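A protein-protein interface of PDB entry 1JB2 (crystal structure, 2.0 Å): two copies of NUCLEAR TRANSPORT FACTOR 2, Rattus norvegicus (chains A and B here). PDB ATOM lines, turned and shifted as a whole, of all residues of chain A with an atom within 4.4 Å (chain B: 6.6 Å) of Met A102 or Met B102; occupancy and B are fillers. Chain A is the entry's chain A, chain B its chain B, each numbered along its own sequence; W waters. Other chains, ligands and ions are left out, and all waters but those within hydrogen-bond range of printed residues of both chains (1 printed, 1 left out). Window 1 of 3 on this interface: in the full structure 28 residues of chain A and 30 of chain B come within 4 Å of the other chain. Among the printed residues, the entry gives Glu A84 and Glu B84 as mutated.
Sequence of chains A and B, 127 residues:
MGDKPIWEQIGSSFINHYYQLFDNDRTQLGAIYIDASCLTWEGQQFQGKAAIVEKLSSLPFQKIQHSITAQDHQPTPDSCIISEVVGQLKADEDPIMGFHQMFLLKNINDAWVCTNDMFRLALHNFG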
ATOM      1  N   SER A  83       1.989   7.107  37.278  1.00  0.00           N
ATOM      2  CA  SER A  83       3.348   6.629  37.466  1.00  0.00           C
ATOM      3  C   SER A  83       3.828   5.741  36.347  1.00  0.00           C
ATOM      4  O   SER A  83       3.050   5.004  35.756  1.00  0.00           O
ATOM      5  CB  SER A  83       3.455   5.843  38.770  1.00  0.00           C
ATOM      6  OG  SER A  83       2.951   6.582  39.855  1.00  0.00           O
ATOM      7  N   GLU A  84       5.131   5.804  36.090  1.00  0.00           N
ATOM      8  CA  GLU A  84       5.752   5.006  35.059  1.00  0.00           C
ATOM      9  C   GLU A  84       6.960   4.261  35.643  1.00  0.00           C
ATOM     10  O   GLU A  84       7.812   4.858  36.302  1.00  0.00           O
ATOM     11  CB  GLU A  84       6.166   5.928  33.897  1.00  0.00           C
ATOM     12  CG  GLU A  84       7.208   5.348  33.005  1.00  0.00           C
ATOM     13  CD  GLU A  84       7.323   6.060  31.674  1.00  0.00           C
ATOM     14  OE1 GLU A  84       7.557   7.288  31.646  1.00  0.00           O
ATOM     15  OE2 GLU A  84       7.194   5.368  30.643  1.00  0.00           O
ATOM     16  N   HIS A 100       7.768  -2.901  31.395  1.00  0.00           N
ATOM     17  CA  HIS A 100       7.347  -1.528  31.598  1.00  0.00           C
ATOM     18  C   HIS A 100       5.980  -1.658  32.266  1.00  0.00           C
ATOM     19  O   HIS A 100       5.220  -2.565  31.946  1.00  0.00           O
ATOM     20  CB  HIS A 100       7.211  -0.801  30.257  1.00  0.00           C
ATOM     21  CG  HIS A 100       7.071   0.680  30.396  1.00  0.00           C
ATOM     22  ND1 HIS A 100       5.977   1.269  30.996  1.00  0.00           N
ATOM     23  CD2 HIS A 100       7.915   1.691  30.076  1.00  0.00           C
ATOM     24  CE1 HIS A 100       6.158   2.578  31.044  1.00  0.00           C
ATOM     25  NE2 HIS A 100       7.325   2.860  30.493  1.00  0.00           N
ATOM     26  N   GLN A 101       5.668  -0.764  33.194  1.00  0.00           N
ATOM     27  CA  GLN A 101       4.380  -0.810  33.848  1.00  0.00           C
ATOM     28  C   GLN A 101       3.929   0.607  34.160  1.00  0.00           C
ATOM     29  O   GLN A 101       4.732   1.449  34.551  1.00  0.00           O
ATOM     30  CB  GLN A 101       4.448  -1.655  35.133  1.00  0.00           C
ATOM     31  CG  GLN A 101       3.079  -1.952  35.760  1.00  0.00           C
ATOM     32  CD  GLN A 101       3.125  -3.183  36.682  1.00  0.00           C
ATOM     33  OE1 GLN A 101       4.203  -3.617  37.096  1.00  0.00           O
ATOM     34  NE2 GLN A 101       1.965  -3.735  37.005  1.00  0.00           N
ATOM     35  N   MET A 102       2.649   0.878  33.936  1.00  0.00           N
ATOM     36  CA  MET A 102       2.078   2.194  34.231  1.00  0.00           C
ATOM     37  C   MET A 102       0.992   2.011  35.255  1.00  0.00           C
ATOM     38  O   MET A 102       0.274   1.014  35.244  1.00  0.00           O
ATOM     39  CB  MET A 102       1.480   2.850  32.989  1.00  0.00           C
ATOM     40  CG  MET A 102       1.157   1.898  31.891  1.00  0.00           C
ATOM     41  SD  MET A 102       1.525   2.556  30.264  1.00  0.00           S
ATOM     42  CE  MET A 102       0.186   3.800  30.066  1.00  0.00           C
ATOM     43  N   PHE A 103       0.869   2.994  36.133  1.00  0.00           N
ATOM     44  CA  PHE A 103      -0.120   2.952  37.194  1.00  0.00           C
ATOM     45  C   PHE A 103      -0.816   4.293  37.276  1.00  0.00           C
ATOM     46  O   PHE A 103      -0.177   5.335  37.140  1.00  0.00           O
ATOM     47  CB  PHE A 103       0.538   2.714  38.571  1.00  0.00           C
ATOM     48  CG  PHE A 103       1.318   1.423  38.685  1.00  0.00           C
ATOM     49  CD1 PHE A 103       2.676   1.384  38.397  1.00  0.00           C
ATOM     50  CD2 PHE A 103       0.689   0.247  39.113  1.00  0.00           C
ATOM     51  CE1 PHE A 103       3.413   0.190  38.539  1.00  0.00           C
ATOM     52  CE2 PHE A 103       1.405  -0.950  39.259  1.00  0.00           C
ATOM     53  CZ  PHE A 103       2.773  -0.974  38.972  1.00  0.00           C
ATOM     54  N   ASN A 116      -5.919   2.086  37.334  1.00  0.00           N
ATOM     55  CA  ASN A 116      -5.527   1.620  36.007  1.00  0.00           C
ATOM     56  C   ASN A 116      -4.083   1.118  36.073  1.00  0.00           C
ATOM     57  O   ASN A 116      -3.188   1.814  36.569  1.00  0.00           O
ATOM     58  CB  ASN A 116      -5.669   2.764  34.985  1.00  0.00           C
ATOM     59  CG  ASN A 116      -7.116   3.246  34.841  1.00  0.00           C
ATOM     60  OD1 ASN A 116      -7.831   2.850  33.906  1.00  0.00           O
ATOM     61  ND2 ASN A 116      -7.555   4.077  35.770  1.00  0.00           N
ATOM     62  N   ASP A 117      -3.877  -0.099  35.573  1.00  0.00           N
ATOM     63  CA  ASP A 117      -2.579  -0.775  35.597  1.00  0.00           C
ATOM     64  C   ASP A 117      -2.315  -1.362  34.211  1.00  0.00           C
ATOM     65  O   ASP A 117      -3.153  -2.092  33.679  1.00  0.00           O
ATOM     66  CB  ASP A 117      -2.657  -1.882  36.663  1.00  0.00           C
ATOM     67  CG  ASP A 117      -1.374  -2.701  36.811  1.00  0.00           C
ATOM     68  OD1 ASP A 117      -0.470  -2.627  35.963  1.00  0.00           O
ATOM     69  OD2 ASP A 117      -1.287  -3.456  37.805  1.00  0.00           O
ATOM     70  N   MET A 118      -1.179  -1.002  33.604  1.00  0.00           N
ATOM     71  CA  MET A 118      -0.802  -1.527  32.284  1.00  0.00           C
ATOM     72  C   MET A 118       0.607  -2.100  32.335  1.00  0.00           C
ATOM     73  O   MET A 118       1.603  -1.365  32.450  1.00  0.00           O
ATOM     74  CB  MET A 118      -0.865  -0.439  31.199  1.00  0.00           C
ATOM     75  CG  MET A 118      -2.286   0.008  30.804  1.00  0.00           C
ATOM     76  SD  MET A 118      -2.258   1.348  29.542  1.00  0.00           S
ATOM     77  CE  MET A 118      -3.991   1.426  29.063  1.00  0.00           C
ATOM     78  N   TYR B  19       0.167  11.914  16.650  1.00  0.00           N
ATOM     79  CA  TYR B  19       1.379  11.662  15.894  1.00  0.00           C
ATOM     80  C   TYR B  19       1.300  12.300  14.514  1.00  0.00           C
ATOM     81  O   TYR B  19       2.319  12.697  13.953  1.00  0.00           O
ATOM     82  CB  TYR B  19       1.650  10.158  15.813  1.00  0.00           C
ATOM     83  CG  TYR B  19       2.032   9.603  17.174  1.00  0.00           C
ATOM     84  CD1 TYR B  19       1.335   8.545  17.739  1.00  0.00           C
ATOM     85  CD2 TYR B  19       3.079  10.162  17.901  1.00  0.00           C
ATOM     86  CE1 TYR B  19       1.666   8.052  18.993  1.00  0.00           C
ATOM     87  CE2 TYR B  19       3.425   9.672  19.164  1.00  0.00           C
ATOM     88  CZ  TYR B  19       2.713   8.616  19.700  1.00  0.00           C
ATOM     89  OH  TYR B  19       3.043   8.124  20.935  1.00  0.00           O
ATOM     90  N   ASP B  72      -2.490   0.400  23.893  1.00  0.00           N
ATOM     91  CA  ASP B  72      -3.511  -0.128  24.798  1.00  0.00           C
ATOM     92  C   ASP B  72      -4.229   1.083  25.403  1.00  0.00           C
ATOM     93  O   ASP B  72      -3.606   2.129  25.618  1.00  0.00           O
ATOM     94  CB  ASP B  72      -2.876  -0.972  25.925  1.00  0.00           C
ATOM     95  CG  ASP B  72      -2.059  -2.160  25.406  1.00  0.00           C
ATOM     96  OD1 ASP B  72      -2.645  -3.153  24.935  1.00  0.00           O
ATOM     97  OD2 ASP B  72      -0.812  -2.109  25.474  1.00  0.00           O
ATOM     98  N   ILE B  82      -6.655   6.458  29.650  1.00  0.00           N
ATOM     99  CA  ILE B  82      -5.217   6.349  29.797  1.00  0.00           C
ATOM    100  C   ILE B  82      -4.795   5.452  28.645  1.00  0.00           C
ATOM    101  O   ILE B  82      -5.433   4.424  28.383  1.00  0.00           O
ATOM    102  CB  ILE B  82      -4.817   5.779  31.198  1.00  0.00           C
ATOM    103  CG1 ILE B  82      -3.304   5.924  31.385  1.00  0.00           C
ATOM    104  CG2 ILE B  82      -5.305   4.336  31.361  1.00  0.00           C
ATOM    105  CD1 ILE B  82      -2.774   5.427  32.743  1.00  0.00           C
ATOM    106  N   SER B  83      -3.754   5.889  27.943  1.00  0.00           N
ATOM    107  CA  SER B  83      -3.244   5.225  26.746  1.00  0.00           C
ATOM    108  C   SER B  83      -1.737   4.978  26.773  1.00  0.00           C
ATOM    109  O   SER B  83      -0.961   5.820  27.221  1.00  0.00           O
ATOM    110  CB  SER B  83      -3.567   6.086  25.516  1.00  0.00           C
ATOM    111  OG  SER B  83      -4.963   6.364  25.418  1.00  0.00           O
ATOM    112  N   GLU B  84      -1.339   3.819  26.264  1.00  0.00           N
ATOM    113  CA  GLU B  84       0.063   3.434  26.202  1.00  0.00           C
ATOM    114  C   GLU B  84       0.383   3.098  24.759  1.00  0.00           C
ATOM    115  O   GLU B  84      -0.421   2.469  24.062  1.00  0.00           O
ATOM    116  CB  GLU B  84       0.314   2.219  27.086  1.00  0.00           C
ATOM    117  CG  GLU B  84       1.687   1.588  26.879  1.00  0.00           C
ATOM    118  CD  GLU B  84       1.937   0.389  27.789  1.00  0.00           C
ATOM    119  OE1 GLU B  84       0.997  -0.385  28.031  1.00  0.00           O
ATOM    120  OE2 GLU B  84       3.091   0.205  28.241  1.00  0.00           O
ATOM    121  N   VAL B  85       1.568   3.506  24.322  1.00  0.00           N
ATOM    122  CA  VAL B  85       2.008   3.294  22.961  1.00  0.00           C
ATOM    123  C   VAL B  85       3.477   2.909  22.953  1.00  0.00           C
ATOM    124  O   VAL B  85       4.268   3.425  23.752  1.00  0.00           O
ATOM    125  CB  VAL B  85       1.823   4.631  22.126  1.00  0.00           C
ATOM    126  CG1 VAL B  85       2.382   4.489  20.733  1.00  0.00           C
ATOM    127  CG2 VAL B  85       0.342   5.000  22.068  1.00  0.00           C
ATOM    128  N   HIS B 100       8.511   4.778  23.883  1.00  0.00           N
ATOM    129  CA  HIS B 100       7.370   4.363  24.648  1.00  0.00           C
ATOM    130  C   HIS B 100       6.679   5.665  25.055  1.00  0.00           C
ATOM    131  O   HIS B 100       7.347   6.630  25.390  1.00  0.00           O
ATOM    132  CB  HIS B 100       7.790   3.585  25.886  1.00  0.00           C
ATOM    133  CG  HIS B 100       6.627   3.127  26.698  1.00  0.00           C
ATOM    134  ND1 HIS B 100       5.884   3.992  27.475  1.00  0.00           N
ATOM    135  CD2 HIS B 100       6.007   1.927  26.767  1.00  0.00           C
ATOM    136  CE1 HIS B 100       4.856   3.342  27.988  1.00  0.00           C
ATOM    137  NE2 HIS B 100       4.906   2.088  27.574  1.00  0.00           N
ATOM    138  N   GLN B 101       5.356   5.710  24.988  1.00  0.00           N
ATOM    139  CA  GLN B 101       4.660   6.925  25.377  1.00  0.00           C
ATOM    140  C   GLN B 101       3.365   6.620  26.109  1.00  0.00           C
ATOM    141  O   GLN B 101       2.669   5.662  25.787  1.00  0.00           O
ATOM    142  CB  GLN B 101       4.381   7.816  24.156  1.00  0.00           C
ATOM    143  CG  GLN B 101       4.023   9.266  24.535  1.00  0.00           C
ATOM    144  CD  GLN B 101       4.247  10.258  23.403  1.00  0.00           C
ATOM    145  OE1 GLN B 101       4.427   9.867  22.249  1.00  0.00           O
ATOM    146  NE2 GLN B 101       4.240  11.556  23.735  1.00  0.00           N
ATOM    147  N   MET B 102       3.050   7.447  27.099  1.00  0.00           N
ATOM    148  CA  MET B 102       1.845   7.274  27.883  1.00  0.00           C
ATOM    149  C   MET B 102       1.080   8.576  27.809  1.00  0.00           C
ATOM    150  O   MET B 102       1.685   9.639  27.864  1.00  0.00           O
ATOM    151  CB  MET B 102       2.200   6.985  29.352  1.00  0.00           C
ATOM    152  CG  MET B 102       3.260   5.893  29.535  1.00  0.00           C
ATOM    153  SD  MET B 102       3.937   5.822  31.228  1.00  0.00           S
ATOM    154  CE  MET B 102       3.682   4.111  31.564  1.00  0.00           C
ATOM    155  N   PHE B 103      -0.245   8.491  27.683  1.00  0.00           N
ATOM    156  CA  PHE B 103      -1.087   9.690  27.642  1.00  0.00           C
ATOM    157  C   PHE B 103      -2.273   9.503  28.563  1.00  0.00           C
ATOM    158  O   PHE B 103      -2.823   8.401  28.619  1.00  0.00           O
ATOM    159  CB  PHE B 103      -1.699   9.933  26.255  1.00  0.00           C
ATOM    160  CG  PHE B 103      -0.711  10.008  25.133  1.00  0.00           C
ATOM    161  CD1 PHE B 103      -0.332   8.850  24.442  1.00  0.00           C
ATOM    162  CD2 PHE B 103      -0.203  11.232  24.726  1.00  0.00           C
ATOM    163  CE1 PHE B 103       0.529   8.927  23.366  1.00  0.00           C
ATOM    164  CE2 PHE B 103       0.665  11.321  23.642  1.00  0.00           C
ATOM    165  CZ  PHE B 103       1.029  10.167  22.959  1.00  0.00           C
ATOM    166  N   LEU B 104      -2.653  10.568  29.270  1.00  0.00           N
ATOM    167  CA  LEU B 104      -3.859  10.593  30.103  1.00  0.00           C
ATOM    168  C   LEU B 104      -4.691  11.668  29.403  1.00  0.00           C
ATOM    169  O   LEU B 104      -4.260  12.827  29.264  1.00  0.00           O
ATOM    170  CB  LEU B 104      -3.599  11.017  31.561  1.00  0.00           C
ATOM    171  CG  LEU B 104      -4.869  10.925  32.436  1.00  0.00           C
ATOM    172  CD1 LEU B 104      -5.449   9.519  32.382  1.00  0.00           C
ATOM    173  CD2 LEU B 104      -4.532  11.276  33.888  1.00  0.00           C
ATOM    174  N   CYS B 114      -4.795  16.251  26.287  1.00  0.00           N
ATOM    175  CA  CYS B 114      -3.851  15.468  27.047  1.00  0.00           C
ATOM    176  C   CYS B 114      -3.452  16.255  28.289  1.00  0.00           C
ATOM    177  O   CYS B 114      -2.949  17.370  28.183  1.00  0.00           O
ATOM    178  CB  CYS B 114      -2.613  15.189  26.197  1.00  0.00           C
ATOM    179  SG  CYS B 114      -1.380  14.246  27.058  1.00  0.00           S
ATOM    180  N   ASN B 116      -1.583  14.586  30.796  1.00  0.00           N
ATOM    181  CA  ASN B 116      -0.323  13.981  31.230  1.00  0.00           C
ATOM    182  C   ASN B 116       0.327  13.214  30.087  1.00  0.00           C
ATOM    183  O   ASN B 116      -0.323  12.406  29.443  1.00  0.00           O
ATOM    184  CB  ASN B 116      -0.587  13.039  32.419  1.00  0.00           C
ATOM    185  CG  ASN B 116      -1.025  13.788  33.687  1.00  0.00           C
ATOM    186  OD1 ASN B 116      -0.190  14.169  34.518  1.00  0.00           O
ATOM    187  ND2 ASN B 116      -2.336  13.999  33.835  1.00  0.00           N
ATOM    188  N   ASP B 117       1.619  13.442  29.876  1.00  0.00           N
ATOM    189  CA  ASP B 117       2.354  12.843  28.772  1.00  0.00           C
ATOM    190  C   ASP B 117       3.714  12.408  29.293  1.00  0.00           C
ATOM    191  O   ASP B 117       4.434  13.216  29.878  1.00  0.00           O
ATOM    192  CB  ASP B 117       2.528  13.931  27.691  1.00  0.00           C
ATOM    193  CG  ASP B 117       3.207  13.442  26.414  1.00  0.00           C
ATOM    194  OD1 ASP B 117       3.813  12.354  26.391  1.00  0.00           O
ATOM    195  OD2 ASP B 117       3.139  14.183  25.410  1.00  0.00           O
ATOM    196  N   MET B 118       4.073  11.138  29.112  1.00  0.00           N
ATOM    197  CA  MET B 118       5.395  10.692  29.559  1.00  0.00           C
ATOM    198  C   MET B 118       6.000   9.958  28.381  1.00  0.00           C
ATOM    199  O   MET B 118       5.377   9.066  27.819  1.00  0.00           O
ATOM    200  CB  MET B 118       5.298   9.797  30.797  1.00  0.00           C
ATOM    201  CG  MET B 118       4.712  10.534  31.988  1.00  0.00           C
ATOM    202  SD  MET B 118       4.344   9.437  33.360  1.00  0.00           S
ATOM    203  CE  MET B 118       5.740   9.637  34.279  1.00  0.00           C
ATOM    204  N   PHE B 119       7.210  10.364  28.014  1.00  0.00           N
ATOM    205  CA  PHE B 119       7.898   9.824  26.859  1.00  0.00           C
ATOM    206  C   PHE B 119       9.298   9.348  27.194  1.00  0.00           C
ATOM    207  O   PHE B 119      10.056  10.045  27.872  1.00  0.00           O
ATOM    208  CB  PHE B 119       7.960  10.912  25.778  1.00  0.00           C
ATOM    209  CG  PHE B 119       8.741  10.518  24.544  1.00  0.00           C
ATOM    210  CD1 PHE B 119       8.109   9.880  23.473  1.00  0.00           C
ATOM    211  CD2 PHE B 119      10.113  10.793  24.454  1.00  0.00           C
ATOM    212  CE1 PHE B 119       8.829   9.521  22.325  1.00  0.00           C
ATOM    213  CE2 PHE B 119      10.845  10.434  23.301  1.00  0.00           C
ATOM    214  CZ  PHE B 119      10.198   9.800  22.242  1.00  0.00           C
HETATM  215  O   HOH W   1       6.625   6.260  28.344  1.00  0.00           O
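The side-chain sulfur of Met B102 sits close to the side-chain carboxylate of Glu A84 (3.3 Å). OE2 of Glu B84 lies close to SD of Met A102, 3.5 Å away.
The side-chain carboxylate of Glu A84 is in hydrogen-bond range of a ring nitrogen (NE2) of His A100 (2.5 Å). N of Met A102 lies within hydrogen-bond range of O of Met A118 (2.9 Å). The backbone carbonyl oxygen (O) of Asp B72 is in hydrogen-bond range of the backbone NH (N) of Glu B84, 2.9 Å away. The backbone NH (N) of Ser B83 lies within hydrogen-bond range of the backbone carbonyl oxygen (O) of Phe B103, 2.8 Å away. A ring nitrogen (NE2) of His B100 is in hydrogen-bond range of the side-chain carboxylate of Glu B84 (2.7 Å). N of Met B102 is in hydrogen-bond range of O of Met B118, 2.9 Å away.
OE2 of Glu A84 touches ND1 of His B100, 3.7 Å away. Met B118 touches Glu A84 (CB to OE1, 3.5 Å). His A100 touches His B100. Met B102 touches His A100. Met A102 touches Ser B83. CB of Met A102 touches CE of Met B102 (2.9 Å). Asn A116 touches Ile B82. Asp B72 touches Met A118 (O to CE, 3.5 Å). Met A118 touches Ile B82. Glu B84 touches Met A118.
Of chain B, only Ser B83, Glu B84 and Met B102 come within 4 Å of Met A102. Of chain A, only Glu A84, His A100 and Met A102 come within 4 Å of Met B102. Printed residues of chain B within 4 Å of Met A118: Asp B72 (3.5 Å), Ile B82 (3.4 Å) and Glu B84 (3.7 Å). Of the printed residues of chain A, Ser B83 touches Met A102. The nearest residue of chain B that does not touch Met A102 is His B100 (4.1 Å). The nearest residue of chain A that does not touch Met B102 is Gln A101 (4.1 Å). The nearest printed residue of chain A that does not touch Ser B83 is Met A118 (4.5 Å).
Of the 16 printed residues of chain B, 7 touch a printed residue of chain A. Hydrophobic or aromatic side chains of chain B within 4 Å of the printed part of chain A: Ile B82, His B100, Met B102 and Met B118. Of the 9 printed residues of chain A, 5 touch a printed residue of chain B. Hydrophobic or aromatic side chains of chain A within 4 Å of the printed part of chain B: His A100, Met A102 and Met A118.
Glu A84 touches His B100, but with the chains exchanged His A100 does not touch Glu B84 (4.1 Å). Glu A84 touches Met B118, and with the chains exchanged Met A118 touches Glu B84. His A100 touches Met B102, but with the chains exchanged Met A102 does not touch His B100 (4.1 Å). Met B102 touches its own counterpart, Met A102. Of the 12 pairs that touch across the chains among the printed residues, 6 have their exchanged pair printed and touching as well.
Water W1 lies within hydrogen-bond range of OE2 of Glu A84 (2.5 Å), ND1 of His B100 (2.5 Å) and O of Met B118 (3.1 Å).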
